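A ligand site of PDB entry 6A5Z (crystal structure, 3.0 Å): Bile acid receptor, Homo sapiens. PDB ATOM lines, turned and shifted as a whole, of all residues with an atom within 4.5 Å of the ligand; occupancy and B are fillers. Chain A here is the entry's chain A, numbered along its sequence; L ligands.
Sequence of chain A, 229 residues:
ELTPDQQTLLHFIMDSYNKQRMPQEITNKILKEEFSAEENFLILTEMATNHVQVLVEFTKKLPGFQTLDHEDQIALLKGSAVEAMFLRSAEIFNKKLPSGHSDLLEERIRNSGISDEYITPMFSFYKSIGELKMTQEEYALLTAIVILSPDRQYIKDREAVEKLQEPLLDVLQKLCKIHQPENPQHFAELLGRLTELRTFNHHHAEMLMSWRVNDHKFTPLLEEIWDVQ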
ATOM      1  N   MET A  22      17.970  15.029  -7.590  1.00  0.00           N
ATOM      2  CA  MET A  22      17.934  13.641  -7.144  1.00  0.00           C
ATOM      3  C   MET A  22      16.442  13.271  -7.034  1.00  0.00           C
ATOM      4  O   MET A  22      15.643  14.081  -6.545  1.00  0.00           O
ATOM      5  CB  MET A  22      18.644  13.482  -5.790  1.00  0.00           C
ATOM      6  CG  MET A  22      18.922  12.043  -5.374  1.00  0.00           C
ATOM      7  SD  MET A  22      20.150  11.205  -6.404  1.00  0.00           S
ATOM      8  CE  MET A  22      21.700  11.627  -5.629  1.00  0.00           C
ATOM      9  N   PHE A  41      26.292   1.272   2.185  1.00  0.00           N
ATOM     10  CA  PHE A  41      27.026   1.190   0.923  1.00  0.00           C
ATOM     11  C   PHE A  41      26.085   1.234  -0.289  1.00  0.00           C
ATOM     12  O   PHE A  41      26.258   2.063  -1.171  1.00  0.00           O
ATOM     13  CB  PHE A  41      27.898  -0.075   0.833  1.00  0.00           C
ATOM     14  CG  PHE A  41      28.499  -0.288  -0.528  1.00  0.00           C
ATOM     15  CD1 PHE A  41      29.653   0.389  -0.909  1.00  0.00           C
ATOM     16  CD2 PHE A  41      27.878  -1.115  -1.458  1.00  0.00           C
ATOM     17  CE1 PHE A  41      30.185   0.213  -2.185  1.00  0.00           C
ATOM     18  CE2 PHE A  41      28.409  -1.288  -2.725  1.00  0.00           C
ATOM     19  CZ  PHE A  41      29.566  -0.617  -3.085  1.00  0.00           C
ATOM     20  N   LEU A  44      24.518   4.787  -1.096  1.00  0.00           N
ATOM     21  CA  LEU A  44      25.527   5.694  -1.663  1.00  0.00           C
ATOM     22  C   LEU A  44      25.797   5.347  -3.113  1.00  0.00           C
ATOM     23  O   LEU A  44      25.801   6.230  -3.954  1.00  0.00           O
ATOM     24  CB  LEU A  44      26.849   5.628  -0.881  1.00  0.00           C
ATOM     25  CG  LEU A  44      26.874   6.002   0.596  1.00  0.00           C
ATOM     26  CD1 LEU A  44      28.292   5.855   1.128  1.00  0.00           C
ATOM     27  CD2 LEU A  44      26.372   7.418   0.813  1.00  0.00           C
ATOM     28  N   THR A  45      25.999   4.066  -3.387  1.00  0.00           N
ATOM     29  CA  THR A  45      26.252   3.574  -4.739  1.00  0.00           C
ATOM     30  C   THR A  45      25.120   3.896  -5.688  1.00  0.00           C
ATOM     31  O   THR A  45      25.347   4.268  -6.842  1.00  0.00           O
ATOM     32  CB  THR A  45      26.526   2.045  -4.744  1.00  0.00           C
ATOM     33  OG1 THR A  45      27.483   1.731  -3.706  1.00  0.00           O
ATOM     34  CG2 THR A  45      27.088   1.605  -6.074  1.00  0.00           C
ATOM     35  N   MET A  47      22.893   6.456  -5.220  1.00  0.00           N
ATOM     36  CA  MET A  47      22.975   7.912  -5.363  1.00  0.00           C
ATOM     37  C   MET A  47      24.089   8.348  -6.300  1.00  0.00           C
ATOM     38  O   MET A  47      23.876   9.183  -7.175  1.00  0.00           O
ATOM     39  CB  MET A  47      23.202   8.587  -4.001  1.00  0.00           C
ATOM     40  CG  MET A  47      22.040   8.512  -3.038  1.00  0.00           C
ATOM     41  SD  MET A  47      22.446   9.486  -1.597  1.00  0.00           S
ATOM     42  CE  MET A  47      21.607  10.993  -2.028  1.00  0.00           C
ATOM     43  N   ALA A  48      25.277   7.776  -6.109  1.00  0.00           N
ATOM     44  CA  ALA A  48      26.455   8.117  -6.917  1.00  0.00           C
ATOM     45  C   ALA A  48      26.262   7.753  -8.366  1.00  0.00           C
ATOM     46  O   ALA A  48      26.738   8.469  -9.246  1.00  0.00           O
ATOM     47  CB  ALA A  48      27.711   7.476  -6.346  1.00  0.00           C
ATOM     48  N   HIS A  51      23.903  10.367  -9.525  1.00  0.00           N
ATOM     49  CA  HIS A  51      24.648  11.630  -9.578  1.00  0.00           C
ATOM     50  C   HIS A  51      25.480  11.753 -10.856  1.00  0.00           C
ATOM     51  O   HIS A  51      25.447  12.801 -11.485  1.00  0.00           O
ATOM     52  CB  HIS A  51      25.524  11.857  -8.344  1.00  0.00           C
ATOM     53  CG  HIS A  51      26.092  13.252  -8.260  1.00  0.00           C
ATOM     54  ND1 HIS A  51      25.378  14.357  -8.658  1.00  0.00           N
ATOM     55  CD2 HIS A  51      27.325  13.690  -7.936  1.00  0.00           C
ATOM     56  CE1 HIS A  51      26.141  15.433  -8.555  1.00  0.00           C
ATOM     57  NE2 HIS A  51      27.319  15.055  -8.093  1.00  0.00           N
ATOM     58  N   MET A  85      31.604  15.742  -7.718  1.00  0.00           N
ATOM     59  CA  MET A  85      30.758  15.069  -6.705  1.00  0.00           C
ATOM     60  C   MET A  85      31.081  15.591  -5.294  1.00  0.00           C
ATOM     61  O   MET A  85      30.176  15.764  -4.477  1.00  0.00           O
ATOM     62  CB  MET A  85      30.848  13.521  -6.759  1.00  0.00           C
ATOM     63  CG  MET A  85      30.952  12.923  -8.164  1.00  0.00           C
ATOM     64  SD  MET A  85      30.084  11.427  -8.608  1.00  0.00           S
ATOM     65  CE  MET A  85      30.393  10.323  -7.277  1.00  0.00           C
ATOM     66  N   PHE A  86      32.362  15.854  -5.020  1.00  0.00           N
ATOM     67  CA  PHE A  86      32.793  16.483  -3.770  1.00  0.00           C
ATOM     68  C   PHE A  86      32.259  17.895  -3.583  1.00  0.00           C
ATOM     69  O   PHE A  86      31.861  18.267  -2.484  1.00  0.00           O
ATOM     70  CB  PHE A  86      34.314  16.494  -3.632  1.00  0.00           C
ATOM     71  CG  PHE A  86      34.867  15.263  -2.978  1.00  0.00           C
ATOM     72  CD1 PHE A  86      35.229  14.152  -3.730  1.00  0.00           C
ATOM     73  CD2 PHE A  86      35.028  15.211  -1.616  1.00  0.00           C
ATOM     74  CE1 PHE A  86      35.742  13.016  -3.124  1.00  0.00           C
ATOM     75  CE2 PHE A  86      35.539  14.085  -1.012  1.00  0.00           C
ATOM     76  CZ  PHE A  86      35.897  12.983  -1.765  1.00  0.00           C
ATOM     77  N   ARG A  88      29.432  19.104  -4.977  1.00  0.00           N
ATOM     78  CA  ARG A  88      27.963  18.994  -4.812  1.00  0.00           C
ATOM     79  C   ARG A  88      27.598  18.442  -3.443  1.00  0.00           C
ATOM     80  O   ARG A  88      26.598  18.837  -2.880  1.00  0.00           O
ATOM     81  CB  ARG A  88      27.326  18.122  -5.907  1.00  0.00           C
ATOM     82  CG  ARG A  88      26.056  18.730  -6.523  1.00  0.00           C
ATOM     83  CD  ARG A  88      24.804  18.659  -5.683  1.00  0.00           C
ATOM     84  NE  ARG A  88      23.990  19.849  -5.924  1.00  0.00           N
ATOM     85  CZ  ARG A  88      22.707  19.989  -5.611  1.00  0.00           C
ATOM     86  NH1 ARG A  88      22.019  19.017  -5.041  1.00  0.00           N
ATOM     87  NH2 ARG A  88      22.091  21.133  -5.893  1.00  0.00           N
ATOM     88  N   SER A  89      28.434  17.555  -2.911  1.00  0.00           N
ATOM     89  CA  SER A  89      28.234  17.005  -1.562  1.00  0.00           C
ATOM     90  C   SER A  89      28.572  17.984  -0.448  1.00  0.00           C
ATOM     91  O   SER A  89      28.033  17.862   0.659  1.00  0.00           O
ATOM     92  CB  SER A  89      29.042  15.719  -1.375  1.00  0.00           C
ATOM     93  OG  SER A  89      30.390  15.975  -1.018  1.00  0.00           O
ATOM     94  N   ILE A  92      25.562  20.201  -0.095  1.00  0.00           N
ATOM     95  CA  ILE A  92      24.593  19.459   0.737  1.00  0.00           C
ATOM     96  C   ILE A  92      24.876  19.658   2.237  1.00  0.00           C
ATOM     97  O   ILE A  92      23.998  20.091   2.987  1.00  0.00           O
ATOM     98  CB  ILE A  92      24.540  17.952   0.330  1.00  0.00           C
ATOM     99  CG1 ILE A  92      24.140  17.767  -1.143  1.00  0.00           C
ATOM    100  CG2 ILE A  92      23.581  17.180   1.207  1.00  0.00           C
ATOM    101  CD1 ILE A  92      22.837  18.405  -1.602  1.00  0.00           C
ATOM    102  N   LEU A 105      22.927  11.233   6.240  1.00  0.00           N
ATOM    103  CA  LEU A 105      23.851  11.021   5.124  1.00  0.00           C
ATOM    104  C   LEU A 105      25.320  11.005   5.542  1.00  0.00           C
ATOM    105  O   LEU A 105      26.071  10.146   5.092  1.00  0.00           O
ATOM    106  CB  LEU A 105      23.668  12.131   4.088  1.00  0.00           C
ATOM    107  CG  LEU A 105      24.597  12.104   2.878  1.00  0.00           C
ATOM    108  CD1 LEU A 105      24.549  10.756   2.178  1.00  0.00           C
ATOM    109  CD2 LEU A 105      24.220  13.213   1.912  1.00  0.00           C
ATOM    110  N   ILE A 109      27.697   7.582   5.313  1.00  0.00           N
ATOM    111  CA  ILE A 109      29.051   7.630   4.763  1.00  0.00           C
ATOM    112  C   ILE A 109      30.090   7.133   5.774  1.00  0.00           C
ATOM    113  O   ILE A 109      30.972   6.344   5.434  1.00  0.00           O
ATOM    114  CB  ILE A 109      29.428   9.062   4.311  1.00  0.00           C
ATOM    115  CG1 ILE A 109      28.581   9.471   3.094  1.00  0.00           C
ATOM    116  CG2 ILE A 109      30.909   9.174   3.963  1.00  0.00           C
ATOM    117  CD1 ILE A 109      28.444  10.968   2.943  1.00  0.00           C
ATOM    118  N   ILE A 114      34.244   2.345   4.634  1.00  0.00           N
ATOM    119  CA  ILE A 114      35.394   3.089   4.109  1.00  0.00           C
ATOM    120  C   ILE A 114      36.519   2.991   5.139  1.00  0.00           C
ATOM    121  O   ILE A 114      36.258   3.041   6.338  1.00  0.00           O
ATOM    122  CB  ILE A 114      35.084   4.590   3.844  1.00  0.00           C
ATOM    123  CG1 ILE A 114      33.860   4.769   2.951  1.00  0.00           C
ATOM    124  CG2 ILE A 114      36.262   5.282   3.165  1.00  0.00           C
ATOM    125  CD1 ILE A 114      33.263   6.157   2.990  1.00  0.00           C
ATOM    126  N   MET A 122      38.136  13.955   4.494  1.00  0.00           N
ATOM    127  CA  MET A 122      36.927  14.169   3.706  1.00  0.00           C
ATOM    128  C   MET A 122      36.046  15.229   4.363  1.00  0.00           C
ATOM    129  O   MET A 122      35.593  16.140   3.707  1.00  0.00           O
ATOM    130  CB  MET A 122      36.167  12.855   3.565  1.00  0.00           C
ATOM    131  CG  MET A 122      35.117  12.830   2.497  1.00  0.00           C
ATOM    132  SD  MET A 122      34.095  11.373   2.564  1.00  0.00           S
ATOM    133  CE  MET A 122      35.308  10.055   2.566  1.00  0.00           C
ATOM    134  N   TYR A 126      34.893  19.484   3.735  1.00  0.00           N
ATOM    135  CA  TYR A 126      33.560  20.084   3.751  1.00  0.00           C
ATOM    136  C   TYR A 126      33.470  21.294   4.668  1.00  0.00           C
ATOM    137  O   TYR A 126      32.725  22.231   4.382  1.00  0.00           O
ATOM    138  CB  TYR A 126      32.477  19.082   4.151  1.00  0.00           C
ATOM    139  CG  TYR A 126      32.376  17.854   3.266  1.00  0.00           C
ATOM    140  CD1 TYR A 126      32.474  17.945   1.877  1.00  0.00           C
ATOM    141  CD2 TYR A 126      32.170  16.606   3.817  1.00  0.00           C
ATOM    142  CE1 TYR A 126      32.385  16.800   1.079  1.00  0.00           C
ATOM    143  CE2 TYR A 126      32.084  15.455   3.040  1.00  0.00           C
ATOM    144  CZ  TYR A 126      32.186  15.573   1.677  1.00  0.00           C
ATOM    145  OH  TYR A 126      32.072  14.449   0.916  1.00  0.00           O
ATOM    146  N   HIS A 204      41.241   8.721  -4.793  1.00  0.00           N
ATOM    147  CA  HIS A 204      39.913   8.098  -4.941  1.00  0.00           C
ATOM    148  C   HIS A 204      39.934   6.650  -5.429  1.00  0.00           C
ATOM    149  O   HIS A 204      39.103   5.862  -5.016  1.00  0.00           O
ATOM    150  CB  HIS A 204      39.016   8.915  -5.867  1.00  0.00           C
ATOM    151  CG  HIS A 204      37.570   8.614  -5.688  1.00  0.00           C
ATOM    152  ND1 HIS A 204      36.801   8.010  -6.669  1.00  0.00           N
ATOM    153  CD2 HIS A 204      36.747   8.792  -4.627  1.00  0.00           C
ATOM    154  CE1 HIS A 204      35.573   7.863  -6.222  1.00  0.00           C
ATOM    155  NE2 HIS A 204      35.513   8.316  -4.984  1.00  0.00           N
ATOM    156  N   MET A 207      40.600   4.453  -2.322  1.00  0.00           N
ATOM    157  CA  MET A 207      39.423   4.422  -1.439  1.00  0.00           C
ATOM    158  C   MET A 207      38.395   3.407  -1.951  1.00  0.00           C
ATOM    159  O   MET A 207      37.834   2.650  -1.155  1.00  0.00           O
ATOM    160  CB  MET A 207      38.765   5.818  -1.320  1.00  0.00           C
ATOM    161  CG  MET A 207      37.643   5.874  -0.279  1.00  0.00           C
ATOM    162  SD  MET A 207      36.819   7.470  -0.076  1.00  0.00           S
ATOM    163  CE  MET A 207      35.924   7.628  -1.604  1.00  0.00           C
ATOM    164  N   LEU A 208      38.159   3.404  -3.262  1.00  0.00           N
ATOM    165  CA  LEU A 208      37.248   2.470  -3.921  1.00  0.00           C
ATOM    166  C   LEU A 208      37.720   1.035  -3.789  1.00  0.00           C
ATOM    167  O   LEU A 208      36.913   0.140  -3.529  1.00  0.00           O
ATOM    168  CB  LEU A 208      37.079   2.790  -5.423  1.00  0.00           C
ATOM    169  CG  LEU A 208      36.364   4.081  -5.845  1.00  0.00           C
ATOM    170  CD1 LEU A 208      36.606   4.348  -7.305  1.00  0.00           C
ATOM    171  CD2 LEU A 208      34.872   3.993  -5.583  1.00  0.00           C
ATOM    172  N   TRP A 211      37.453  -0.110  -0.096  1.00  0.00           N
ATOM    173  CA  TRP A 211      36.091  -0.023   0.450  1.00  0.00           C
ATOM    174  C   TRP A 211      35.618  -1.420   0.844  1.00  0.00           C
ATOM    175  O   TRP A 211      35.866  -2.382   0.106  1.00  0.00           O
ATOM    176  CB  TRP A 211      35.145   0.545  -0.603  1.00  0.00           C
ATOM    177  CG  TRP A 211      33.978   1.271  -0.050  1.00  0.00           C
ATOM    178  CD1 TRP A 211      33.083   0.831   0.868  1.00  0.00           C
ATOM    179  CD2 TRP A 211      33.561   2.584  -0.414  1.00  0.00           C
ATOM    180  NE1 TRP A 211      32.152   1.782   1.127  1.00  0.00           N
ATOM    181  CE2 TRP A 211      32.411   2.878   0.350  1.00  0.00           C
ATOM    182  CE3 TRP A 211      34.050   3.547  -1.298  1.00  0.00           C
ATOM    183  CZ2 TRP A 211      31.730   4.099   0.246  1.00  0.00           C
ATOM    184  CZ3 TRP A 211      33.381   4.763  -1.391  1.00  0.00           C
ATOM    185  CH2 TRP A 211      32.240   5.028  -0.622  1.00  0.00           C
ATOM    186  N   PHE A 218      30.772  -2.118  -7.979  1.00  0.00           N
ATOM    187  CA  PHE A 218      29.960  -0.953  -7.666  1.00  0.00           C
ATOM    188  C   PHE A 218      28.746  -1.043  -8.602  1.00  0.00           C
ATOM    189  O   PHE A 218      27.854  -1.857  -8.347  1.00  0.00           O
ATOM    190  CB  PHE A 218      30.786   0.339  -7.806  1.00  0.00           C
ATOM    191  CG  PHE A 218      31.889   0.465  -6.786  1.00  0.00           C
ATOM    192  CD1 PHE A 218      33.154  -0.079  -7.026  1.00  0.00           C
ATOM    193  CD2 PHE A 218      31.679   1.111  -5.583  1.00  0.00           C
ATOM    194  CE1 PHE A 218      34.174  -0.001  -6.079  1.00  0.00           C
ATOM    195  CE2 PHE A 218      32.693   1.208  -4.640  1.00  0.00           C
ATOM    196  CZ  PHE A 218      33.942   0.647  -4.887  1.00  0.00           C
ATOM    197  N   LEU A 222      29.569   3.497 -12.697  1.00  0.00           N
ATOM    198  CA  LEU A 222      30.678   3.879 -11.795  1.00  0.00           C
ATOM    199  C   LEU A 222      31.961   3.078 -12.079  1.00  0.00           C
ATOM    200  O   LEU A 222      33.050   3.623 -11.979  1.00  0.00           O
ATOM    201  CB  LEU A 222      30.283   3.748 -10.329  1.00  0.00           C
ATOM    202  CG  LEU A 222      29.095   4.611  -9.853  1.00  0.00           C
ATOM    203  CD1 LEU A 222      28.896   4.416  -8.355  1.00  0.00           C
ATOM    204  CD2 LEU A 222      29.266   6.095 -10.162  1.00  0.00           C
ATOM    205  N   TRP A 226      35.280   5.445 -13.173  1.00  0.00           N
ATOM    206  CA  TRP A 226      36.515   5.249 -12.389  1.00  0.00           C
ATOM    207  C   TRP A 226      37.397   4.022 -12.690  1.00  0.00           C
ATOM    208  O   TRP A 226      38.416   3.834 -12.040  1.00  0.00           O
ATOM    209  CB  TRP A 226      36.159   5.242 -10.885  1.00  0.00           C
ATOM    210  CG  TRP A 226      35.441   6.494 -10.477  1.00  0.00           C
ATOM    211  CD1 TRP A 226      35.671   7.743 -10.947  1.00  0.00           C
ATOM    212  CD2 TRP A 226      34.382   6.605  -9.527  1.00  0.00           C
ATOM    213  NE1 TRP A 226      34.831   8.645 -10.353  1.00  0.00           N
ATOM    214  CE2 TRP A 226      34.022   7.969  -9.472  1.00  0.00           C
ATOM    215  CE3 TRP A 226      33.700   5.691  -8.703  1.00  0.00           C
ATOM    216  CZ2 TRP A 226      33.019   8.457  -8.631  1.00  0.00           C
ATOM    217  CZ3 TRP A 226      32.699   6.169  -7.861  1.00  0.00           C
ATOM    218  CH2 TRP A 226      32.368   7.537  -7.837  1.00  0.00           C
HETATM  219  O1  LIG L   1      20.186  17.260  -5.209  1.00  0.00           O
HETATM  220  C1  LIG L   1      20.069  16.793  -4.057  1.00  0.00           C
HETATM  221  O2  LIG L   1      19.057  17.034  -3.334  1.00  0.00           O
HETATM  222  C2  LIG L   1      21.144  15.862  -3.567  1.00  0.00           C
HETATM  223  C3  LIG L   1      20.997  15.336  -2.283  1.00  0.00           C
HETATM  224  C4  LIG L   1      21.927  14.442  -1.770  1.00  0.00           C
HETATM  225  C5  LIG L   1      23.022  14.048  -2.536  1.00  0.00           C
HETATM  226  N1  LIG L   1      24.019  13.181  -2.210  1.00  0.00           N
HETATM  227  C6  LIG L   1      22.246  15.473  -4.375  1.00  0.00           C
HETATM  228  C7  LIG L   1      23.172  14.559  -3.848  1.00  0.00           C
HETATM  229  S1  LIG L   1      24.563  13.990  -4.651  1.00  0.00           S
HETATM  230  C8  LIG L   1      24.920  13.066  -3.221  1.00  0.00           C
HETATM  231  N2  LIG L   1      25.965  12.206  -3.161  1.00  0.00           N
HETATM  232  C9  LIG L   1      26.253  11.543  -1.870  1.00  0.00           C
HETATM  233  C10 LIG L   1      26.577  11.893  -4.452  1.00  0.00           C
HETATM  234  C11 LIG L   1      27.927  11.262  -4.259  1.00  0.00           C
HETATM  235  C12 LIG L   1      28.933  12.335  -3.860  1.00  0.00           C
HETATM  236  C13 LIG L   1      28.876  12.706  -2.382  1.00  0.00           C
HETATM  237  C14 LIG L   1      28.625  11.576  -1.405  1.00  0.00           C
HETATM  238  C15 LIG L   1      27.509  10.698  -1.892  1.00  0.00           C
HETATM  239  C16 LIG L   1      27.851  10.144  -3.263  1.00  0.00           C
HETATM  240  O3  LIG L   1      29.163   9.574  -3.315  1.00  0.00           O
HETATM  241  C17 LIG L   1      29.240   8.286  -2.735  1.00  0.00           C
HETATM  242  C18 LIG L   1      30.587   7.767  -3.080  1.00  0.00           C
HETATM  243  C19 LIG L   1      30.888   6.434  -3.558  1.00  0.00           C
HETATM  244  C20 LIG L   1      30.051   5.258  -3.867  1.00  0.00           C
HETATM  245  C21 LIG L   1      30.601   3.879  -3.491  1.00  0.00           C
HETATM  246  C22 LIG L   1      30.624   4.336  -4.956  1.00  0.00           C
HETATM  247  O4  LIG L   1      32.226   6.416  -3.751  1.00  0.00           O
HETATM  248  C23 LIG L   1      31.916   8.448  -3.024  1.00  0.00           C
HETATM  249  N3  LIG L   1      32.865   7.560  -3.427  1.00  0.00           N
HETATM  250  C24 LIG L   1      32.137   9.845  -2.556  1.00  0.00           C
HETATM  251  C25 LIG L   1      31.979  10.109  -1.212  1.00  0.00           C
HETATM  252 CL1  LIG L   1      31.536   8.708  -0.197  1.00  0.00          CL
HETATM  253  C26 LIG L   1      32.128  11.398  -0.704  1.00  0.00           C
HETATM  254  C27 LIG L   1      32.465  12.424  -1.580  1.00  0.00           C
HETATM  255  C28 LIG L   1      32.624  12.158  -2.933  1.00  0.00           C
HETATM  256  C29 LIG L   1      32.464  10.868  -3.431  1.00  0.00           C
HETATM  257 CL2  LIG L   1      32.669  10.522  -5.177  1.00  0.00          CL
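The guanidinium group (NH1) of Arg 88 lies within salt-bridge range of an oxygen (O1) of the ligand (2.5 Å).
NE2 of His 204 lies within hydrogen-bond range of N3 of the ligand, at 3.2 Å.
O of Phe 86 is in hydrogen-bond range of OG of Ser 89 (3.1 Å).
OG1 of Thr 45 sits at hydrogen-bond distance from O of Phe 41 (2.8 Å).
O of Met 85 lies close to OG of Ser 89, at 3.5 Å.
The side-chain hydroxyl (OG) of Ser 89 sits at hydrogen-bond distance from the side-chain hydroxyl (OH) of Tyr 126, at 3.0 Å.
Met 22 touches the ligand (CE to C7, 3.7 Å).
Phe 41 touches the ligand (CE1 to C21, 3.9 Å).
OG1 of Thr 45 touches C21 of the ligand, 3.8 Å away.
Met 47 touches the ligand (CE to N1, 3.3 Å).
Ala 48 touches the ligand (CB to O3, 3.96 Å).
CG of His 51 touches S1 of the ligand (3.99 Å).
Met 85 touches the ligand.
Phe 86 touches the ligand (CE1 to C28, 3.2 Å).
CB of Ser 89 touches C13 of the ligand (3.2 Å).
Ile 92 touches the ligand.
Met 122 touches the ligand.
OH of Tyr 126 touches C27 of the ligand, 3.2 Å away.
CE of Met 207 touches N3 of the ligand (3.6 Å).
Trp 211 touches the ligand (CZ3 to O4, 3.1 Å).
Phe 218 touches the ligand.
Leu 222 touches the ligand.
Hydrophobic or aromatic side chains that line the ligand: Met 22, Phe 41, Met 47, Ala 48, His 51, Met 85, Phe 86, Ile 92, Met 122, His 204, Met 207, Trp 211, Phe 218 and Leu 222.
18 residues have an atom within 4 Å of the ligand: Met 22, Phe 41, Thr 45, Met 47, Ala 48, His 51, Met 85, Phe 86, Arg 88, Ser 89, Ile 92, Met 122, Tyr 126, His 204, Met 207, Trp 211, Phe 218 and Leu 222.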
